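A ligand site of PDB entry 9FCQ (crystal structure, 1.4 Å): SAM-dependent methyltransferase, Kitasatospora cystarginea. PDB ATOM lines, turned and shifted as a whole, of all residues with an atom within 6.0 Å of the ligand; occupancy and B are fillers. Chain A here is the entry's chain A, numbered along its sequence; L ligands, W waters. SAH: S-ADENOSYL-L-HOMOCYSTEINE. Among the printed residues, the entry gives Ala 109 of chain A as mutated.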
ATOM      1  N   TYR A   4      25.706 -39.294 -12.128  1.00  0.00           N
ATOM      2  CA  TYR A   4      25.635 -38.291 -11.040  1.00  0.00           C
ATOM      3  C   TYR A   4      24.605 -38.762 -10.009  1.00  0.00           C
ATOM      4  O   TYR A   4      24.894 -38.720  -8.802  1.00  0.00           O
ATOM      5  CB  TYR A   4      25.257 -36.892 -11.557  1.00  0.00           C
ATOM      6  CG  TYR A   4      24.965 -35.901 -10.470  1.00  0.00           C
ATOM      7  CD1 TYR A   4      25.950 -35.079  -9.957  1.00  0.00           C
ATOM      8  CD2 TYR A   4      23.701 -35.813  -9.899  1.00  0.00           C
ATOM      9  CE1 TYR A   4      25.693 -34.179  -8.944  1.00  0.00           C
ATOM     10  CE2 TYR A   4      23.421 -34.919  -8.877  1.00  0.00           C
ATOM     11  CZ  TYR A   4      24.427 -34.106  -8.399  1.00  0.00           C
ATOM     12  OH  TYR A   4      24.157 -33.225  -7.382  1.00  0.00           O
ATOM     13  N   ARG A   8      25.086 -39.831  -6.063  1.00  0.00           N
ATOM     14  CA  ARG A   8      24.261 -39.309  -4.946  1.00  0.00           C
ATOM     15  C   ARG A   8      23.755 -40.480  -4.111  1.00  0.00           C
ATOM     16  O   ARG A   8      23.793 -40.374  -2.866  1.00  0.00           O
ATOM     17  CB  ARG A   8      23.131 -38.413  -5.469  1.00  0.00           C
ATOM     18  CG  ARG A   8      23.589 -37.188  -6.240  1.00  0.00           C
ATOM     19  CD  ARG A   8      24.607 -36.340  -5.479  1.00  0.00           C
ATOM     20  NE  ARG A   8      24.012 -35.735  -4.304  1.00  0.00           N
ATOM     21  CZ  ARG A   8      24.692 -35.103  -3.345  1.00  0.00           C
ATOM     22  NH1 ARG A   8      26.003 -35.009  -3.398  1.00  0.00           N
ATOM     23  NH2 ARG A   8      24.028 -34.576  -2.333  1.00  0.00           N
ATOM     24  N   TYR A  19      14.214 -39.633  -0.012  1.00  0.00           N
ATOM     25  CA  TYR A  19      13.635 -38.878  -1.160  1.00  0.00           C
ATOM     26  C   TYR A  19      12.218 -39.409  -1.433  1.00  0.00           C
ATOM     27  O   TYR A  19      11.308 -38.598  -1.695  1.00  0.00           O
ATOM     28  CB  TYR A  19      14.526 -38.962  -2.391  1.00  0.00           C
ATOM     29  CG  TYR A  19      15.680 -37.995  -2.388  1.00  0.00           C
ATOM     30  CD1 TYR A  19      15.668 -36.875  -3.194  1.00  0.00           C
ATOM     31  CD2 TYR A  19      16.767 -38.184  -1.550  1.00  0.00           C
ATOM     32  CE1 TYR A  19      16.727 -35.972  -3.199  1.00  0.00           C
ATOM     33  CE2 TYR A  19      17.824 -37.295  -1.543  1.00  0.00           C
ATOM     34  CZ  TYR A  19      17.804 -36.189  -2.368  1.00  0.00           C
ATOM     35  OH  TYR A  19      18.870 -35.326  -2.354  1.00  0.00           O
ATOM     36  N   ASP A  38      10.939 -26.180  -5.371  1.00  0.00           N
ATOM     37  CA  ASP A  38      12.114 -26.979  -4.951  1.00  0.00           C
ATOM     38  C   ASP A  38      13.234 -25.982  -4.625  1.00  0.00           C
ATOM     39  O   ASP A  38      13.801 -25.431  -5.575  1.00  0.00           O
ATOM     40  CB  ASP A  38      12.488 -28.013  -6.015  1.00  0.00           C
ATOM     41  CG  ASP A  38      13.566 -28.978  -5.579  1.00  0.00           C
ATOM     42  OD1 ASP A  38      13.968 -28.913  -4.401  1.00  0.00           O
ATOM     43  OD2 ASP A  38      13.997 -29.802  -6.427  1.00  0.00           O
ATOM     44  N   LEU A  39      13.490 -25.745  -3.331  1.00  0.00           N
ATOM     45  CA  LEU A  39      14.479 -24.765  -2.804  1.00  0.00           C
ATOM     46  C   LEU A  39      15.861 -25.417  -2.779  1.00  0.00           C
ATOM     47  O   LEU A  39      15.998 -26.466  -2.129  1.00  0.00           O
ATOM     48  CB  LEU A  39      14.081 -24.340  -1.384  1.00  0.00           C
ATOM     49  CG  LEU A  39      13.253 -23.068  -1.252  1.00  0.00           C
ATOM     50  CD1 LEU A  39      12.994 -22.767   0.221  1.00  0.00           C
ATOM     51  CD2 LEU A  39      13.948 -21.892  -1.922  1.00  0.00           C
ATOM     52  N   GLY A  40      16.857 -24.806  -3.412  1.00  0.00           N
ATOM     53  CA  GLY A  40      18.195 -25.409  -3.568  1.00  0.00           C
ATOM     54  C   GLY A  40      18.128 -26.678  -4.397  1.00  0.00           C
ATOM     55  O   GLY A  40      18.754 -27.675  -4.009  1.00  0.00           O
ATOM     56  N   ALA A  41      17.399 -26.616  -5.518  1.00  0.00           N
ATOM     57  CA  ALA A  41      17.017 -27.777  -6.356  1.00  0.00           C
ATOM     58  C   ALA A  41      18.268 -28.457  -6.923  1.00  0.00           C
ATOM     59  O   ALA A  41      18.155 -29.633  -7.315  1.00  0.00           O
ATOM     60  CB  ALA A  41      16.105 -27.321  -7.463  1.00  0.00           C
ATOM     61  N   GLY A  42      19.386 -27.740  -7.045  1.00  0.00           N
ATOM     62  CA  GLY A  42      20.611 -28.285  -7.645  1.00  0.00           C
ATOM     63  C   GLY A  42      20.341 -28.783  -9.047  1.00  0.00           C
ATOM     64  O   GLY A  42      19.792 -28.011  -9.863  1.00  0.00           O
ATOM     65  N   THR A  43      20.648 -30.051  -9.327  1.00  0.00           N
ATOM     66  CA  THR A  43      20.433 -30.695 -10.652  1.00  0.00           C
ATOM     67  C   THR A  43      18.957 -31.094 -10.807  1.00  0.00           C
ATOM     68  O   THR A  43      18.635 -31.638 -11.862  1.00  0.00           O
ATOM     69  CB  THR A  43      21.332 -31.925 -10.832  1.00  0.00           C
ATOM     70  OG1 THR A  43      20.858 -32.950  -9.974  1.00  0.00           O
ATOM     71  CG2 THR A  43      22.798 -31.638 -10.560  1.00  0.00           C
ATOM     72  N   GLY A  44      18.127 -30.859  -9.792  1.00  0.00           N
ATOM     73  CA  GLY A  44      16.662 -31.048  -9.852  1.00  0.00           C
ATOM     74  C   GLY A  44      16.229 -32.444  -9.435  1.00  0.00           C
ATOM     75  O   GLY A  44      15.115 -32.850  -9.795  1.00  0.00           O
ATOM     76  N   LEU A  45      17.046 -33.148  -8.645  1.00  0.00           N
ATOM     77  CA  LEU A  45      16.823 -34.555  -8.248  1.00  0.00           C
ATOM     78  C   LEU A  45      15.490 -34.692  -7.503  1.00  0.00           C
ATOM     79  O   LEU A  45      14.710 -35.594  -7.840  1.00  0.00           O
ATOM     80  CB  LEU A  45      17.993 -35.017  -7.385  1.00  0.00           C
ATOM     81  CG  LEU A  45      18.275 -36.524  -7.360  1.00  0.00           C
ATOM     82  CD1 LEU A  45      18.236 -37.134  -8.754  1.00  0.00           C
ATOM     83  CD2 LEU A  45      19.620 -36.787  -6.705  1.00  0.00           C
ATOM     84  N   LEU A  46      15.217 -33.822  -6.526  1.00  0.00           N
ATOM     85  CA  LEU A  46      13.961 -33.930  -5.737  1.00  0.00           C
ATOM     86  C   LEU A  46      12.771 -33.543  -6.626  1.00  0.00           C
ATOM     87  O   LEU A  46      11.767 -34.259  -6.620  1.00  0.00           O
ATOM     88  CB  LEU A  46      14.024 -33.069  -4.475  1.00  0.00           C
ATOM     89  CG  LEU A  46      12.791 -33.148  -3.570  1.00  0.00           C
ATOM     90  CD1 LEU A  46      12.439 -34.593  -3.243  1.00  0.00           C
ATOM     91  CD2 LEU A  46      12.995 -32.346  -2.303  1.00  0.00           C
ATOM     92  N   GLN A  62      14.536 -23.688  -7.782  1.00  0.00           N
ATOM     93  CA  GLN A  62      15.288 -22.493  -7.367  1.00  0.00           C
ATOM     94  C   GLN A  62      16.622 -22.912  -6.769  1.00  0.00           C
ATOM     95  O   GLN A  62      16.675 -23.861  -5.970  1.00  0.00           O
ATOM     96  CB  GLN A  62      14.495 -21.648  -6.376  1.00  0.00           C
ATOM     97  CG  GLN A  62      15.233 -20.391  -5.972  1.00  0.00           C
ATOM     98  CD  GLN A  62      14.348 -19.482  -5.159  1.00  0.00           C
ATOM     99  OE1 GLN A  62      13.363 -18.954  -5.662  1.00  0.00           O
ATOM    100  NE2 GLN A  62      14.695 -19.300  -3.898  1.00  0.00           N
ATOM    101  N   ASP A  63      17.690 -22.205  -7.139  1.00  0.00           N
ATOM    102  CA  ASP A  63      19.047 -22.441  -6.610  1.00  0.00           C
ATOM    103  C   ASP A  63      19.847 -21.169  -6.844  1.00  0.00           C
ATOM    104  O   ASP A  63      19.482 -20.404  -7.748  1.00  0.00           O
ATOM    105  CB  ASP A  63      19.700 -23.636  -7.307  1.00  0.00           C
ATOM    106  CG  ASP A  63      20.780 -24.306  -6.485  1.00  0.00           C
ATOM    107  OD1 ASP A  63      20.498 -25.378  -5.921  1.00  0.00           O
ATOM    108  OD2 ASP A  63      21.896 -23.761  -6.434  1.00  0.00           O
ATOM    109  N   ARG A  64      20.920 -20.967  -6.079  1.00  0.00           N
ATOM    110  CA  ARG A  64      21.833 -19.818  -6.315  1.00  0.00           C
ATOM    111  C   ARG A  64      22.801 -20.168  -7.452  1.00  0.00           C
ATOM    112  O   ARG A  64      23.383 -19.231  -8.007  1.00  0.00           O
ATOM    113  CB  ARG A  64      22.587 -19.451  -5.040  1.00  0.00           C
ATOM    114  CG  ARG A  64      23.601 -20.477  -4.577  1.00  0.00           C
ATOM    115  CD  ARG A  64      24.324 -19.943  -3.362  1.00  0.00           C
ATOM    116  NE  ARG A  64      25.205 -20.925  -2.761  1.00  0.00           N
ATOM    117  CZ  ARG A  64      25.767 -20.810  -1.565  1.00  0.00           C
ATOM    118  NH1 ARG A  64      25.529 -19.746  -0.811  1.00  0.00           N
ATOM    119  NH2 ARG A  64      26.559 -21.772  -1.104  1.00  0.00           N
ATOM    120  N   SER A  65      22.981 -21.458  -7.776  1.00  0.00           N
ATOM    121  CA  SER A  65      24.010 -21.926  -8.731  1.00  0.00           C
ATOM    122  C   SER A  65      23.410 -22.142 -10.129  1.00  0.00           C
ATOM    123  O   SER A  65      22.653 -23.103 -10.300  1.00  0.00           O
ATOM    124  CB  SER A  65      24.695 -23.171  -8.249  1.00  0.00           C
ATOM    125  OG  SER A  65      25.531 -23.702  -9.259  1.00  0.00           O
ATOM    126  N   MET A  68      24.601 -25.676 -11.381  1.00  0.00           N
ATOM    127  CA  MET A  68      23.729 -26.790 -10.903  1.00  0.00           C
ATOM    128  C   MET A  68      22.422 -26.760 -11.717  1.00  0.00           C
ATOM    129  O   MET A  68      21.993 -27.832 -12.192  1.00  0.00           O
ATOM    130  CB  MET A  68      23.418 -26.661  -9.406  1.00  0.00           C
ATOM    131  CG  MET A  68      24.641 -26.818  -8.530  1.00  0.00           C
ATOM    132  SD  MET A  68      25.374 -28.467  -8.632  1.00  0.00           S
ATOM    133  CE  MET A  68      24.143 -29.427  -7.760  1.00  0.00           C
ATOM    134  N   ALA A  87      18.159 -17.723  -7.386  1.00  0.00           N
ATOM    135  CA  ALA A  87      18.012 -16.925  -6.155  1.00  0.00           C
ATOM    136  C   ALA A  87      18.650 -17.671  -4.988  1.00  0.00           C
ATOM    137  O   ALA A  87      18.559 -18.911  -4.928  1.00  0.00           O
ATOM    138  CB  ALA A  87      16.562 -16.623  -5.894  1.00  0.00           C
ATOM    139  N   ASP A  88      19.274 -16.911  -4.083  1.00  0.00           N
ATOM    140  CA  ASP A  88      19.800 -17.421  -2.800  1.00  0.00           C
ATOM    141  C   ASP A  88      18.598 -17.687  -1.884  1.00  0.00           C
ATOM    142  O   ASP A  88      17.588 -16.970  -2.021  1.00  0.00           O
ATOM    143  CB  ASP A  88      20.773 -16.425  -2.185  1.00  0.00           C
ATOM    144  CG  ASP A  88      21.711 -17.059  -1.182  1.00  0.00           C
ATOM    145  OD1 ASP A  88      22.865 -17.320  -1.561  1.00  0.00           O
ATOM    146  OD2 ASP A  88      21.278 -17.302  -0.035  1.00  0.00           O
ATOM    147  N   HIS A  89      18.709 -18.659  -0.981  1.00  0.00           N
ATOM    148  CA  HIS A  89      17.726 -18.877   0.109  1.00  0.00           C
ATOM    149  C   HIS A  89      17.461 -17.547   0.830  1.00  0.00           C
ATOM    150  O   HIS A  89      16.323 -17.367   1.296  1.00  0.00           O
ATOM    151  CB  HIS A  89      18.206 -19.913   1.123  1.00  0.00           C
ATOM    152  CG  HIS A  89      18.469 -21.265   0.537  1.00  0.00           C
ATOM    153  ND1 HIS A  89      17.843 -21.721  -0.593  1.00  0.00           N
ATOM    154  CD2 HIS A  89      19.289 -22.258   0.957  1.00  0.00           C
ATOM    155  CE1 HIS A  89      18.266 -22.933  -0.863  1.00  0.00           C
ATOM    156  NE2 HIS A  89      19.159 -23.286   0.069  1.00  0.00           N
ATOM    157  N   LEU A  90      18.472 -16.678   0.940  1.00  0.00           N
ATOM    158  CA  LEU A  90      18.410 -15.423   1.736  1.00  0.00           C
ATOM    159  C   LEU A  90      17.746 -14.299   0.922  1.00  0.00           C
ATOM    160  O   LEU A  90      17.360 -13.290   1.529  1.00  0.00           O
ATOM    161  CB  LEU A  90      19.832 -15.028   2.161  1.00  0.00           C
ATOM    162  CG  LEU A  90      20.560 -16.047   3.035  1.00  0.00           C
ATOM    163  CD1 LEU A  90      21.906 -15.494   3.491  1.00  0.00           C
ATOM    164  CD2 LEU A  90      19.724 -16.450   4.234  1.00  0.00           C
ATOM    165  N   SER A 103      12.802 -29.171  -0.192  1.00  0.00           N
ATOM    166  CA  SER A 103      14.256 -28.939  -0.252  1.00  0.00           C
ATOM    167  C   SER A 103      14.958 -30.243   0.094  1.00  0.00           C
ATOM    168  O   SER A 103      14.438 -30.980   0.942  1.00  0.00           O
ATOM    169  CB  SER A 103      14.634 -27.832   0.682  1.00  0.00           C
ATOM    170  OG  SER A 103      15.958 -27.401   0.427  1.00  0.00           O
ATOM    171  N   ALA A 104      16.080 -30.513  -0.557  1.00  0.00           N
ATOM    172  CA  ALA A 104      16.927 -31.671  -0.253  1.00  0.00           C
ATOM    173  C   ALA A 104      18.387 -31.225  -0.135  1.00  0.00           C
ATOM    174  O   ALA A 104      18.920 -30.664  -1.123  1.00  0.00           O
ATOM    175  CB  ALA A 104      16.755 -32.744  -1.297  1.00  0.00           C
ATOM    176  N   LEU A 105      18.972 -31.418   1.053  1.00  0.00           N
ATOM    177  CA  LEU A 105      20.433 -31.337   1.335  1.00  0.00           C
ATOM    178  C   LEU A 105      20.963 -29.957   0.940  1.00  0.00           C
ATOM    179  O   LEU A 105      22.036 -29.892   0.314  1.00  0.00           O
ATOM    180  CB  LEU A 105      21.140 -32.460   0.578  1.00  0.00           C
ATOM    181  CG  LEU A 105      20.628 -33.866   0.875  1.00  0.00           C
ATOM    182  CD1 LEU A 105      21.377 -34.900   0.050  1.00  0.00           C
ATOM    183  CD2 LEU A 105      20.728 -34.176   2.365  1.00  0.00           C
ATOM    184  N   SER A 106      20.258 -28.895   1.324  1.00  0.00           N
ATOM    185  CA  SER A 106      20.585 -27.509   0.917  1.00  0.00           C
ATOM    186  C   SER A 106      20.582 -26.559   2.130  1.00  0.00           C
ATOM    187  O   SER A 106      21.517 -25.753   2.245  1.00  0.00           O
ATOM    188  CB  SER A 106      19.627 -27.039  -0.137  1.00  0.00           C
ATOM    189  OG  SER A 106      20.045 -25.787  -0.652  1.00  0.00           O
ATOM    190  N   ALA A 109      23.358 -25.490   4.855  1.00  0.00           N
ATOM    191  CA  ALA A 109      24.438 -24.544   4.469  1.00  0.00           C
ATOM    192  C   ALA A 109      24.266 -23.200   5.184  1.00  0.00           C
ATOM    193  O   ALA A 109      25.275 -22.471   5.292  1.00  0.00           O
ATOM    194  CB  ALA A 109      24.449 -24.367   2.974  1.00  0.00           C
ATOM    195  N   LEU A 110      23.051 -22.876   5.654  1.00  0.00           N
ATOM    196  CA  LEU A 110      22.715 -21.543   6.236  1.00  0.00           C
ATOM    197  C   LEU A 110      23.081 -21.497   7.723  1.00  0.00           C
ATOM    198  O   LEU A 110      23.011 -22.544   8.382  1.00  0.00           O
ATOM    199  CB  LEU A 110      21.213 -21.271   6.073  1.00  0.00           C
ATOM    200  CG  LEU A 110      20.683 -21.202   4.652  1.00  0.00           C
ATOM    201  CD1 LEU A 110      19.179 -20.932   4.674  1.00  0.00           C
ATOM    202  CD2 LEU A 110      21.390 -20.144   3.829  1.00  0.00           C
HETATM  203  N   SAH L   1      18.504 -30.498  -3.851  1.00  0.00           N
HETATM  204  CA  SAH L   1      19.516 -31.099  -4.769  1.00  0.00           C
HETATM  205  CB  SAH L   1      20.900 -30.471  -4.583  1.00  0.00           C
HETATM  206  CG  SAH L   1      21.546 -30.693  -3.225  1.00  0.00           C
HETATM  207  SD  SAH L   1      23.214 -29.994  -3.140  1.00  0.00           S
HETATM  208  C   SAH L   1      19.580 -32.615  -4.544  1.00  0.00           C
HETATM  209  O   SAH L   1      18.821 -33.124  -3.724  1.00  0.00           O
HETATM  210  OXT SAH L   1      20.376 -33.297  -5.187  1.00  0.00           O
HETATM  211  C5' SAH L   1      22.951 -28.388  -2.356  1.00  0.00           C
HETATM  212  C4' SAH L   1      22.390 -27.344  -3.293  1.00  0.00           C
HETATM  213  O4' SAH L   1      22.055 -26.168  -2.511  1.00  0.00           O
HETATM  214  C3' SAH L   1      23.349 -26.867  -4.389  1.00  0.00           C
HETATM  215  O3' SAH L   1      22.695 -26.892  -5.653  1.00  0.00           O
HETATM  216  C2' SAH L   1      23.734 -25.459  -3.947  1.00  0.00           C
HETATM  217  O2' SAH L   1      24.028 -24.583  -5.011  1.00  0.00           O
HETATM  218  C1' SAH L   1      22.464 -25.028  -3.219  1.00  0.00           C
HETATM  219  N9  SAH L   1      22.637 -23.962  -2.237  1.00  0.00           N
HETATM  220  C8  SAH L   1      23.489 -23.956  -1.163  1.00  0.00           C
HETATM  221  N7  SAH L   1      23.388 -22.868  -0.431  1.00  0.00           N
HETATM  222  C5  SAH L   1      22.407 -22.116  -1.057  1.00  0.00           C
HETATM  223  C6  SAH L   1      21.843 -20.862  -0.767  1.00  0.00           C
HETATM  224  N6  SAH L   1      22.196 -20.120   0.274  1.00  0.00           N
HETATM  225  N1  SAH L   1      20.880 -20.402  -1.601  1.00  0.00           N
HETATM  226  C2  SAH L   1      20.520 -21.162  -2.647  1.00  0.00           C
HETATM  227  N3  SAH L   1      20.973 -22.359  -3.019  1.00  0.00           N
HETATM  228  C4  SAH L   1      21.926 -22.788  -2.167  1.00  0.00           C
HETATM  229  O   HOH W   1      16.330 -31.142  -5.948  1.00  0.00           O
HETATM  230  O   HOH W   2      21.536 -32.353  -7.451  1.00  0.00           O
HETATM  231  O   HOH W   3      24.395 -30.978  -0.195  1.00  0.00           O
HETATM  232  O   HOH W   4      17.107 -20.705  -3.262  1.00  0.00           O
HETATM  233  O   HOH W   5      26.146 -22.830  -4.672  1.00  0.00           O
HETATM  234  O   HOH W   6      21.312 -35.364  -3.722  1.00  0.00           O
HETATM  235  O   HOH W   7      16.232 -29.085  -3.069  1.00  0.00           O
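N7 of the ligand lies close to NH2 of Arg 64 (3.4 Å).
The side-chain carboxylate of Asp 88 sits at hydrogen-bond distance from a nitrogen (N6) of the ligand (3.0 Å).
O of Gly 40 is in hydrogen-bond range of N of the ligand, 2.8 Å away.
O of Ala 104 is in hydrogen-bond range of N of the ligand, 2.8 Å away.
An oxygen (O3') of the ligand is in hydrogen-bond range of the side-chain carboxylate (OD1) of Asp 63, at 2.7 Å.
ND1 of His 89 sits close to N1 of the ligand, at 3.5 Å.
The side-chain hydroxyl (OG) of Ser 106 is in hydrogen-bond range of an oxygen (O4') of the ligand, 2.8 Å away.
The backbone NH of Arg 64 is in hydrogen-bond range of a nitrogen (N3) of the ligand, 3.4 Å away.
OH of Tyr 19 is in hydrogen-bond range of O of the ligand, 2.6 Å away.
N1 of the ligand sits at hydrogen-bond distance from N of His 89, at 2.9 Å.
O of Gln 62 is in hydrogen-bond range of N of Ala 41, at 2.9 Å.
The backbone NH (N) of Gly 40 is in hydrogen-bond range of the backbone carbonyl oxygen (O) of Gln 62 (2.7 Å).
The guanidinium group (NH1) of Arg 64 is in salt-bridge range of the side-chain carboxylate (OD1) of Asp 88, at 3.7 Å.
OD2 of Asp 88 lies close to N of Leu 90 (3.0 Å).
O of Asp 63 is in hydrogen-bond range of N of Ala 87 (3.0 Å).
OD1 of Asp 63 sits at hydrogen-bond distance from N of Gly 42, 2.8 Å away.
N of Met 68 is in hydrogen-bond range of OG of Ser 65 (3.0 Å).
The side-chain carboxylate (OD1) of Asp 63 is in hydrogen-bond range of the backbone NH (N) of Ala 41.
The backbone carbonyl oxygen (O) of Leu 105 lies close to a sulfur (SD) of the ligand (3.7 Å).
Residues that only touch the ligand: Ala 41 (3.2 Å), Gly 42 (3.2 Å), Leu 45 (3.7 Å), Ser 65 (3.6 Å), Met 68 (3.5 Å), Ala 87 (3.8 Å), Ala 109 (3.9 Å) and Leu 110 (3.6 Å).
17 residues have an atom within 4 Å of the ligand: Tyr 19, Gly 40, Ala 41, Gly 42, Leu 45, Asp 63, Arg 64, Ser 65, Met 68, Ala 87, Asp 88, His 89, Ala 104, Leu 105, Ser 106, Ala 109 and Leu 110.
Water W6 lies within hydrogen-bond range of an oxygen (OXT) of the ligand, the guanidinium group of Arg 8 and the side-chain hydroxyl of Tyr 19.
Water W2 lies within hydrogen-bond range of the side-chain hydroxyl of Thr 43 (2.7 Å), an oxygen (OXT) of the ligand (2.7 Å) and the side-chain hydroxyl of Tyr 4 (2.8 Å).
Water W5 bridges O2' of the ligand (2.8 Å) and NE of Arg 64 (2.9 Å).
Water W1 lies within hydrogen-bond range of OD2 of Asp 38, O of Ala 41, N of Leu 46, N of the ligand and N of Leu 45.
Water W3 bridges O of Leu 105 and SD of the ligand.
Water W4 lies within hydrogen-bond range of the backbone carbonyl oxygen (O) of Ala 87 (2.8 Å), the side-chain amide nitrogen (NE2) of Gln 62 (2.9 Å) and a ring nitrogen (ND1) of His 89 (2.9 Å).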
